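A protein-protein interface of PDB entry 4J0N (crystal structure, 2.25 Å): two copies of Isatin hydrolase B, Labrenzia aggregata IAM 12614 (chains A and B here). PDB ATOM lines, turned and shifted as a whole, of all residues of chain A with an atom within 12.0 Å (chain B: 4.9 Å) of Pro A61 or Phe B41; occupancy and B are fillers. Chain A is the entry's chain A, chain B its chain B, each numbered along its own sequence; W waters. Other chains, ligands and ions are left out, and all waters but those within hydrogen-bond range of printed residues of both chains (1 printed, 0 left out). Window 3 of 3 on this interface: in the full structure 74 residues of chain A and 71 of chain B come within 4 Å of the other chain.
Of the 8 printed residues of chain B, 5 touch a printed residue of chain A. Among the printed residues, 10 pairs touch across the chains. Among the printed residues, Asp or Glu carboxylates within 4 Å of a Lys or Arg side-chain nitrogen of the other chain: Asp A59 with Lys B43 (3.0 Å).
The side-chain hydroxyl (OG) of Ser A54 is in hydrogen-bond range of the backbone carbonyl oxygen (O) of Gly A60, 3.4 Å away. The backbone carbonyl oxygen of Phe A63 sits at hydrogen-bond distance from the side-chain hydroxyl of Ser A54, at 3.0 Å. O of Ser A54 lies within hydrogen-bond range of N of Trp A65, at 3.1 Å. The backbone carbonyl oxygen (O) of Phe A63 lies within hydrogen-bond range of the backbone NH (N) of Tyr A56, 2.9 Å away. The backbone carbonyl oxygen of Trp A65 sits at hydrogen-bond distance from the backbone NH of Ile A53 (2.9 Å). The side-chain carboxylate (OD1) of Asp A57 lies within hydrogen-bond range of the backbone NH (N) of Asp A59, at 2.9 Å.
Among the printed residues, pairs that only touch across the chains: Asp A59 with Ala B42 (3.3 Å), Tyr A56 with Ile B85 (3.4 Å), Pro A61 with Phe B41 (3.5 Å), Trp A65 with Lys B43 (3.6 Å), Phe A63 with Ala B42 (3.7 Å), Trp A65 with Leu B37 (3.7 Å), Gly A60 with Ala B42 (3.8 Å) and Phe A63 with Phe B41 (3.8 Å).
Water W1 lies within hydrogen-bond range of the backbone carbonyl oxygen of Asp A59 (2.5 Å), the backbone carbonyl oxygen of Lys B43 (2.8 Å) and the indole nitrogen of Trp A65 (3.0 Å).
No position is printed for both chains.
O of Phe A62 sits at hydrogen-bond distance from N of Ile B85. The side-chain carboxylate (OD1) of Asp A59 lies within salt-bridge range of the side-chain amino group (NZ) of Lys B43 (3.0 Å).
Ser A54 touches none of the printed residues of chain B. Of the printed residues of chain B, Gly A60 touches Ala B42. Of chain B, only Phe B41 comes within 4 Å of Pro A61. Printed residues of chain B within 4 Å of Phe A62: Ile B85 (3.0 Å). Printed residues of chain B within 4 Å of Phe A63: Phe B41 and Ala B42. Printed residues of chain B within 4 Å of Trp A65: Leu B37 (3.7 Å) and Lys B43 (3.6 Å). No residue of chain A comes within 4 Å of Pro B38. Pro B39 touches none of the printed residues of chain A. No residue of chain A comes within 4 Å of Asp B40. Of chain A, only Pro A61 (3.5 Å) and Phe A63 (3.8 Å) come within 4 Å of Phe B41. Of chain A, only Asp A59 and Trp A65 come within 4 Å of Lys B43. The nearest residue of chain B that does not touch Pro A61 is Ile B85 (4.2 Å). The nearest residue of chain A that does not touch Phe B41 is Phe A62 (4.4 Å).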
ATOM      1  N   LYS A  52     -16.576  32.623  21.456  1.00  0.00           N
ATOM      2  CA  LYS A  52     -16.085  31.352  20.915  1.00  0.00           C
ATOM      3  C   LYS A  52     -16.344  30.185  21.871  1.00  0.00           C
ATOM      4  O   LYS A  52     -16.189  30.326  23.086  1.00  0.00           O
ATOM      5  CB  LYS A  52     -14.587  31.445  20.579  1.00  0.00           C
ATOM      6  CG  LYS A  52     -13.892  30.090  20.490  1.00  0.00           C
ATOM      7  CD  LYS A  52     -12.527  30.174  19.794  1.00  0.00           C
ATOM      8  CE  LYS A  52     -11.439  30.684  20.727  1.00  0.00           C
ATOM      9  NZ  LYS A  52     -10.099  30.606  20.072  1.00  0.00           N
ATOM     10  N   ILE A  53     -16.775  29.046  21.332  1.00  0.00           N
ATOM     11  CA  ILE A  53     -16.835  27.826  22.129  1.00  0.00           C
ATOM     12  C   ILE A  53     -15.585  27.008  21.839  1.00  0.00           C
ATOM     13  O   ILE A  53     -14.953  26.459  22.743  1.00  0.00           O
ATOM     14  CB  ILE A  53     -18.048  26.968  21.786  1.00  0.00           C
ATOM     15  CG1 ILE A  53     -19.352  27.748  22.038  1.00  0.00           C
ATOM     16  CG2 ILE A  53     -18.008  25.668  22.587  1.00  0.00           C
ATOM     17  CD1 ILE A  53     -20.604  27.018  21.533  1.00  0.00           C
ATOM     18  N   SER A  54     -15.241  26.936  20.562  1.00  0.00           N
ATOM     19  CA  SER A  54     -14.031  26.266  20.113  1.00  0.00           C
ATOM     20  C   SER A  54     -13.799  26.612  18.654  1.00  0.00           C
ATOM     21  O   SER A  54     -14.719  27.068  17.954  1.00  0.00           O
ATOM     22  CB  SER A  54     -14.152  24.750  20.261  1.00  0.00           C
ATOM     23  OG  SER A  54     -14.884  24.196  19.179  1.00  0.00           O
ATOM     24  N   GLU A  55     -12.566  26.406  18.206  1.00  0.00           N
ATOM     25  CA  GLU A  55     -12.210  26.570  16.804  1.00  0.00           C
ATOM     26  C   GLU A  55     -11.110  25.570  16.490  1.00  0.00           C
ATOM     27  O   GLU A  55      -9.934  25.931  16.412  1.00  0.00           O
ATOM     28  CB  GLU A  55     -11.745  28.001  16.511  1.00  0.00           C
ATOM     29  CG  GLU A  55     -11.523  28.283  15.029  1.00  0.00           C
ATOM     30  CD  GLU A  55     -11.403  29.765  14.727  1.00  0.00           C
ATOM     31  OE1 GLU A  55     -10.906  30.511  15.606  1.00  0.00           O
ATOM     32  OE2 GLU A  55     -11.814  30.181  13.612  1.00  0.00           O
ATOM     33  N   TYR A  56     -11.506  24.310  16.321  1.00  0.00           N
ATOM     34  CA  TYR A  56     -10.573  23.209  16.048  1.00  0.00           C
ATOM     35  C   TYR A  56      -9.422  23.203  17.051  1.00  0.00           C
ATOM     36  O   TYR A  56      -8.254  23.193  16.662  1.00  0.00           O
ATOM     37  CB  TYR A  56     -10.001  23.294  14.630  1.00  0.00           C
ATOM     38  CG  TYR A  56     -10.882  23.970  13.599  1.00  0.00           C
ATOM     39  CD1 TYR A  56     -12.136  23.458  13.273  1.00  0.00           C
ATOM     40  CD2 TYR A  56     -10.438  25.095  12.921  1.00  0.00           C
ATOM     41  CE1 TYR A  56     -12.938  24.075  12.312  1.00  0.00           C
ATOM     42  CE2 TYR A  56     -11.230  25.718  11.962  1.00  0.00           C
ATOM     43  CZ  TYR A  56     -12.476  25.203  11.661  1.00  0.00           C
ATOM     44  OH  TYR A  56     -13.260  25.817  10.706  1.00  0.00           O
ATOM     45  N   ASP A  57      -9.767  23.231  18.336  1.00  0.00           N
ATOM     46  CA  ASP A  57      -8.781  23.261  19.407  1.00  0.00           C
ATOM     47  C   ASP A  57      -9.147  22.280  20.525  1.00  0.00           C
ATOM     48  O   ASP A  57     -10.005  21.413  20.347  1.00  0.00           O
ATOM     49  CB  ASP A  57      -8.603  24.692  19.944  1.00  0.00           C
ATOM     50  CG  ASP A  57      -9.928  25.357  20.339  1.00  0.00           C
ATOM     51  OD1 ASP A  57     -10.733  24.734  21.076  1.00  0.00           O
ATOM     52  OD2 ASP A  57     -10.160  26.520  19.915  1.00  0.00           O
ATOM     53  N   SER A  58      -8.502  22.418  21.679  1.00  0.00           N
ATOM     54  CA  SER A  58      -8.711  21.460  22.765  1.00  0.00           C
ATOM     55  C   SER A  58     -10.098  21.593  23.402  1.00  0.00           C
ATOM     56  O   SER A  58     -10.503  20.747  24.207  1.00  0.00           O
ATOM     57  CB  SER A  58      -7.597  21.574  23.818  1.00  0.00           C
ATOM     58  OG  SER A  58      -7.536  22.880  24.364  1.00  0.00           O
ATOM     59  N   ASP A  59     -10.821  22.655  23.047  1.00  0.00           N
ATOM     60  CA  ASP A  59     -12.192  22.862  23.537  1.00  0.00           C
ATOM     61  C   ASP A  59     -13.225  22.185  22.626  1.00  0.00           C
ATOM     62  O   ASP A  59     -14.391  22.037  22.998  1.00  0.00           O
ATOM     63  CB  ASP A  59     -12.500  24.361  23.657  1.00  0.00           C
ATOM     64  CG  ASP A  59     -11.815  25.013  24.846  1.00  0.00           C
ATOM     65  OD1 ASP A  59     -11.880  24.441  25.957  1.00  0.00           O
ATOM     66  OD2 ASP A  59     -11.218  26.100  24.666  1.00  0.00           O
ATOM     67  N   GLY A  60     -12.777  21.792  21.434  1.00  0.00           N
ATOM     68  CA  GLY A  60     -13.602  21.125  20.434  1.00  0.00           C
ATOM     69  C   GLY A  60     -12.777  20.837  19.185  1.00  0.00           C
ATOM     70  O   GLY A  60     -12.729  21.670  18.276  1.00  0.00           O
ATOM     71  N   PRO A  61     -12.123  19.653  19.135  1.00  0.00           N
ATOM     72  CA  PRO A  61     -11.037  19.281  18.200  1.00  0.00           C
ATOM     73  C   PRO A  61     -11.352  19.360  16.702  1.00  0.00           C
ATOM     74  O   PRO A  61     -10.498  19.792  15.920  1.00  0.00           O
ATOM     75  CB  PRO A  61     -10.727  17.822  18.572  1.00  0.00           C
ATOM     76  CG  PRO A  61     -11.242  17.659  19.967  1.00  0.00           C
ATOM     77  CD  PRO A  61     -12.452  18.552  20.059  1.00  0.00           C
ATOM     78  N   PHE A  62     -12.548  18.935  16.308  1.00  0.00           N
ATOM     79  CA  PHE A  62     -12.879  18.816  14.889  1.00  0.00           C
ATOM     80  C   PHE A  62     -13.859  19.876  14.404  1.00  0.00           C
ATOM     81  O   PHE A  62     -14.364  19.786  13.279  1.00  0.00           O
ATOM     82  CB  PHE A  62     -13.472  17.435  14.610  1.00  0.00           C
ATOM     83  CG  PHE A  62     -12.601  16.311  15.057  1.00  0.00           C
ATOM     84  CD1 PHE A  62     -11.226  16.393  14.914  1.00  0.00           C
ATOM     85  CD2 PHE A  62     -13.149  15.176  15.631  1.00  0.00           C
ATOM     86  CE1 PHE A  62     -10.410  15.353  15.328  1.00  0.00           C
ATOM     87  CE2 PHE A  62     -12.337  14.128  16.054  1.00  0.00           C
ATOM     88  CZ  PHE A  62     -10.967  14.216  15.901  1.00  0.00           C
ATOM     89  N   PHE A  63     -14.128  20.880  15.234  1.00  0.00           N
ATOM     90  CA  PHE A  63     -15.188  21.821  14.890  1.00  0.00           C
ATOM     91  C   PHE A  63     -15.013  23.238  15.442  1.00  0.00           C
ATOM     92  O   PHE A  63     -14.248  23.468  16.377  1.00  0.00           O
ATOM     93  CB  PHE A  63     -16.558  21.250  15.287  1.00  0.00           C
ATOM     94  CG  PHE A  63     -16.571  20.556  16.625  1.00  0.00           C
ATOM     95  CD1 PHE A  63     -16.269  19.203  16.724  1.00  0.00           C
ATOM     96  CD2 PHE A  63     -16.900  21.251  17.779  1.00  0.00           C
ATOM     97  CE1 PHE A  63     -16.278  18.555  17.951  1.00  0.00           C
ATOM     98  CE2 PHE A  63     -16.919  20.611  19.012  1.00  0.00           C
ATOM     99  CZ  PHE A  63     -16.602  19.257  19.095  1.00  0.00           C
ATOM    100  N   ALA A  64     -15.726  24.184  14.834  1.00  0.00           N
ATOM    101  CA  ALA A  64     -15.755  25.555  15.310  1.00  0.00           C
ATOM    102  C   ALA A  64     -17.207  25.938  15.504  1.00  0.00           C
ATOM    103  O   ALA A  64     -18.064  25.601  14.674  1.00  0.00           O
ATOM    104  CB  ALA A  64     -15.097  26.485  14.314  1.00  0.00           C
ATOM    105  N   TRP A  65     -17.480  26.624  16.609  1.00  0.00           N
ATOM    106  CA  TRP A  65     -18.817  27.152  16.891  1.00  0.00           C
ATOM    107  C   TRP A  65     -18.767  28.205  18.006  1.00  0.00           C
ATOM    108  O   TRP A  65     -17.754  28.333  18.720  1.00  0.00           O
ATOM    109  CB  TRP A  65     -19.841  26.033  17.194  1.00  0.00           C
ATOM    110  CG  TRP A  65     -19.430  25.044  18.257  1.00  0.00           C
ATOM    111  CD1 TRP A  65     -18.192  24.922  18.848  1.00  0.00           C
ATOM    112  CD2 TRP A  65     -20.262  24.037  18.860  1.00  0.00           C
ATOM    113  NE1 TRP A  65     -18.216  23.906  19.776  1.00  0.00           N
ATOM    114  CE2 TRP A  65     -19.469  23.347  19.803  1.00  0.00           C
ATOM    115  CE3 TRP A  65     -21.596  23.650  18.690  1.00  0.00           C
ATOM    116  CZ2 TRP A  65     -19.969  22.291  20.575  1.00  0.00           C
ATOM    117  CZ3 TRP A  65     -22.093  22.602  19.460  1.00  0.00           C
ATOM    118  CH2 TRP A  65     -21.280  21.934  20.393  1.00  0.00           C
ATOM    119  N   LEU B  37     -22.271  16.773  24.540  1.00  0.00           N
ATOM    120  CA  LEU B  37     -21.042  16.059  24.197  1.00  0.00           C
ATOM    121  C   LEU B  37     -20.340  15.536  25.459  1.00  0.00           C
ATOM    122  O   LEU B  37     -20.572  16.051  26.559  1.00  0.00           O
ATOM    123  CB  LEU B  37     -20.087  16.985  23.426  1.00  0.00           C
ATOM    124  CG  LEU B  37     -20.500  17.422  22.018  1.00  0.00           C
ATOM    125  CD1 LEU B  37     -19.794  18.721  21.643  1.00  0.00           C
ATOM    126  CD2 LEU B  37     -20.214  16.331  20.979  1.00  0.00           C
ATOM    127  N   PRO B  38     -19.482  14.506  25.303  1.00  0.00           N
ATOM    128  CA  PRO B  38     -18.630  14.054  26.417  1.00  0.00           C
ATOM    129  C   PRO B  38     -17.753  15.197  26.899  1.00  0.00           C
ATOM    130  O   PRO B  38     -17.005  15.779  26.109  1.00  0.00           O
ATOM    131  CB  PRO B  38     -17.742  12.982  25.776  1.00  0.00           C
ATOM    132  CG  PRO B  38     -18.519  12.492  24.582  1.00  0.00           C
ATOM    133  CD  PRO B  38     -19.310  13.682  24.089  1.00  0.00           C
ATOM    134  N   PRO B  39     -17.836  15.518  28.192  1.00  0.00           N
ATOM    135  CA  PRO B  39     -17.129  16.685  28.752  1.00  0.00           C
ATOM    136  C   PRO B  39     -15.600  16.572  28.729  1.00  0.00           C
ATOM    137  O   PRO B  39     -14.928  17.596  28.869  1.00  0.00           O
ATOM    138  CB  PRO B  39     -17.655  16.769  30.194  1.00  0.00           C
ATOM    139  CG  PRO B  39     -18.173  15.387  30.505  1.00  0.00           C
ATOM    140  CD  PRO B  39     -18.656  14.812  29.194  1.00  0.00           C
ATOM    141  N   ASP B  40     -15.067  15.360  28.570  1.00  0.00           N
ATOM    142  CA  ASP B  40     -13.630  15.166  28.394  1.00  0.00           C
ATOM    143  C   ASP B  40     -13.264  15.201  26.913  1.00  0.00           C
ATOM    144  O   ASP B  40     -12.107  14.991  26.542  1.00  0.00           O
ATOM    145  CB  ASP B  40     -13.171  13.841  29.019  1.00  0.00           C
ATOM    146  CG  ASP B  40     -12.991  13.934  30.527  1.00  0.00           C
ATOM    147  OD1 ASP B  40     -12.509  14.982  31.014  1.00  0.00           O
ATOM    148  OD2 ASP B  40     -13.329  12.958  31.229  1.00  0.00           O
ATOM    149  N   PHE B  41     -14.258  15.462  26.070  1.00  0.00           N
ATOM    150  CA  PHE B  41     -14.030  15.547  24.635  1.00  0.00           C
ATOM    151  C   PHE B  41     -14.107  16.977  24.101  1.00  0.00           C
ATOM    152  O   PHE B  41     -13.352  17.341  23.196  1.00  0.00           O
ATOM    153  CB  PHE B  41     -15.019  14.662  23.871  1.00  0.00           C
ATOM    154  CG  PHE B  41     -14.987  14.871  22.381  1.00  0.00           C
ATOM    155  CD1 PHE B  41     -13.830  14.597  21.651  1.00  0.00           C
ATOM    156  CD2 PHE B  41     -16.108  15.345  21.708  1.00  0.00           C
ATOM    157  CE1 PHE B  41     -13.792  14.795  20.267  1.00  0.00           C
ATOM    158  CE2 PHE B  41     -16.087  15.546  20.330  1.00  0.00           C
ATOM    159  CZ  PHE B  41     -14.926  15.271  19.604  1.00  0.00           C
ATOM    160  N   ALA B  42     -15.027  17.774  24.648  1.00  0.00           N
ATOM    161  CA  ALA B  42     -15.288  19.130  24.149  1.00  0.00           C
ATOM    162  C   ALA B  42     -16.221  19.941  25.064  1.00  0.00           C
ATOM    163  O   ALA B  42     -16.958  19.377  25.882  1.00  0.00           O
ATOM    164  CB  ALA B  42     -15.865  19.068  22.728  1.00  0.00           C
ATOM    165  N   LYS B  43     -16.190  21.265  24.925  1.00  0.00           N
ATOM    166  CA  LYS B  43     -17.087  22.115  25.702  1.00  0.00           C
ATOM    167  C   LYS B  43     -18.501  22.083  25.101  1.00  0.00           C
ATOM    168  O   LYS B  43     -18.669  21.875  23.900  1.00  0.00           O
ATOM    169  CB  LYS B  43     -16.549  23.550  25.781  1.00  0.00           C
ATOM    170  CG  LYS B  43     -15.112  23.661  26.312  1.00  0.00           C
ATOM    171  CD  LYS B  43     -14.969  23.076  27.734  1.00  0.00           C
ATOM    172  CE  LYS B  43     -13.513  23.105  28.254  1.00  0.00           C
ATOM    173  NZ  LYS B  43     -12.594  22.097  27.616  1.00  0.00           N
ATOM    174  N   ILE B  85     -13.722  21.143  10.695  1.00  0.00           N
ATOM    175  CA  ILE B  85     -12.327  21.281  10.283  1.00  0.00           C
ATOM    176  C   ILE B  85     -12.161  21.050   8.778  1.00  0.00           C
ATOM    177  O   ILE B  85     -11.399  21.748   8.114  1.00  0.00           O
ATOM    178  CB  ILE B  85     -11.390  20.382  11.147  1.00  0.00           C
ATOM    179  CG1 ILE B  85      -9.917  20.742  10.921  1.00  0.00           C
ATOM    180  CG2 ILE B  85     -11.642  18.904  10.902  1.00  0.00           C
ATOM    181  CD1 ILE B  85      -9.009  20.238  12.026  1.00  0.00           C
HETATM  182  O   HOH W   1     -16.676  22.412  21.937  1.00  0.00           O
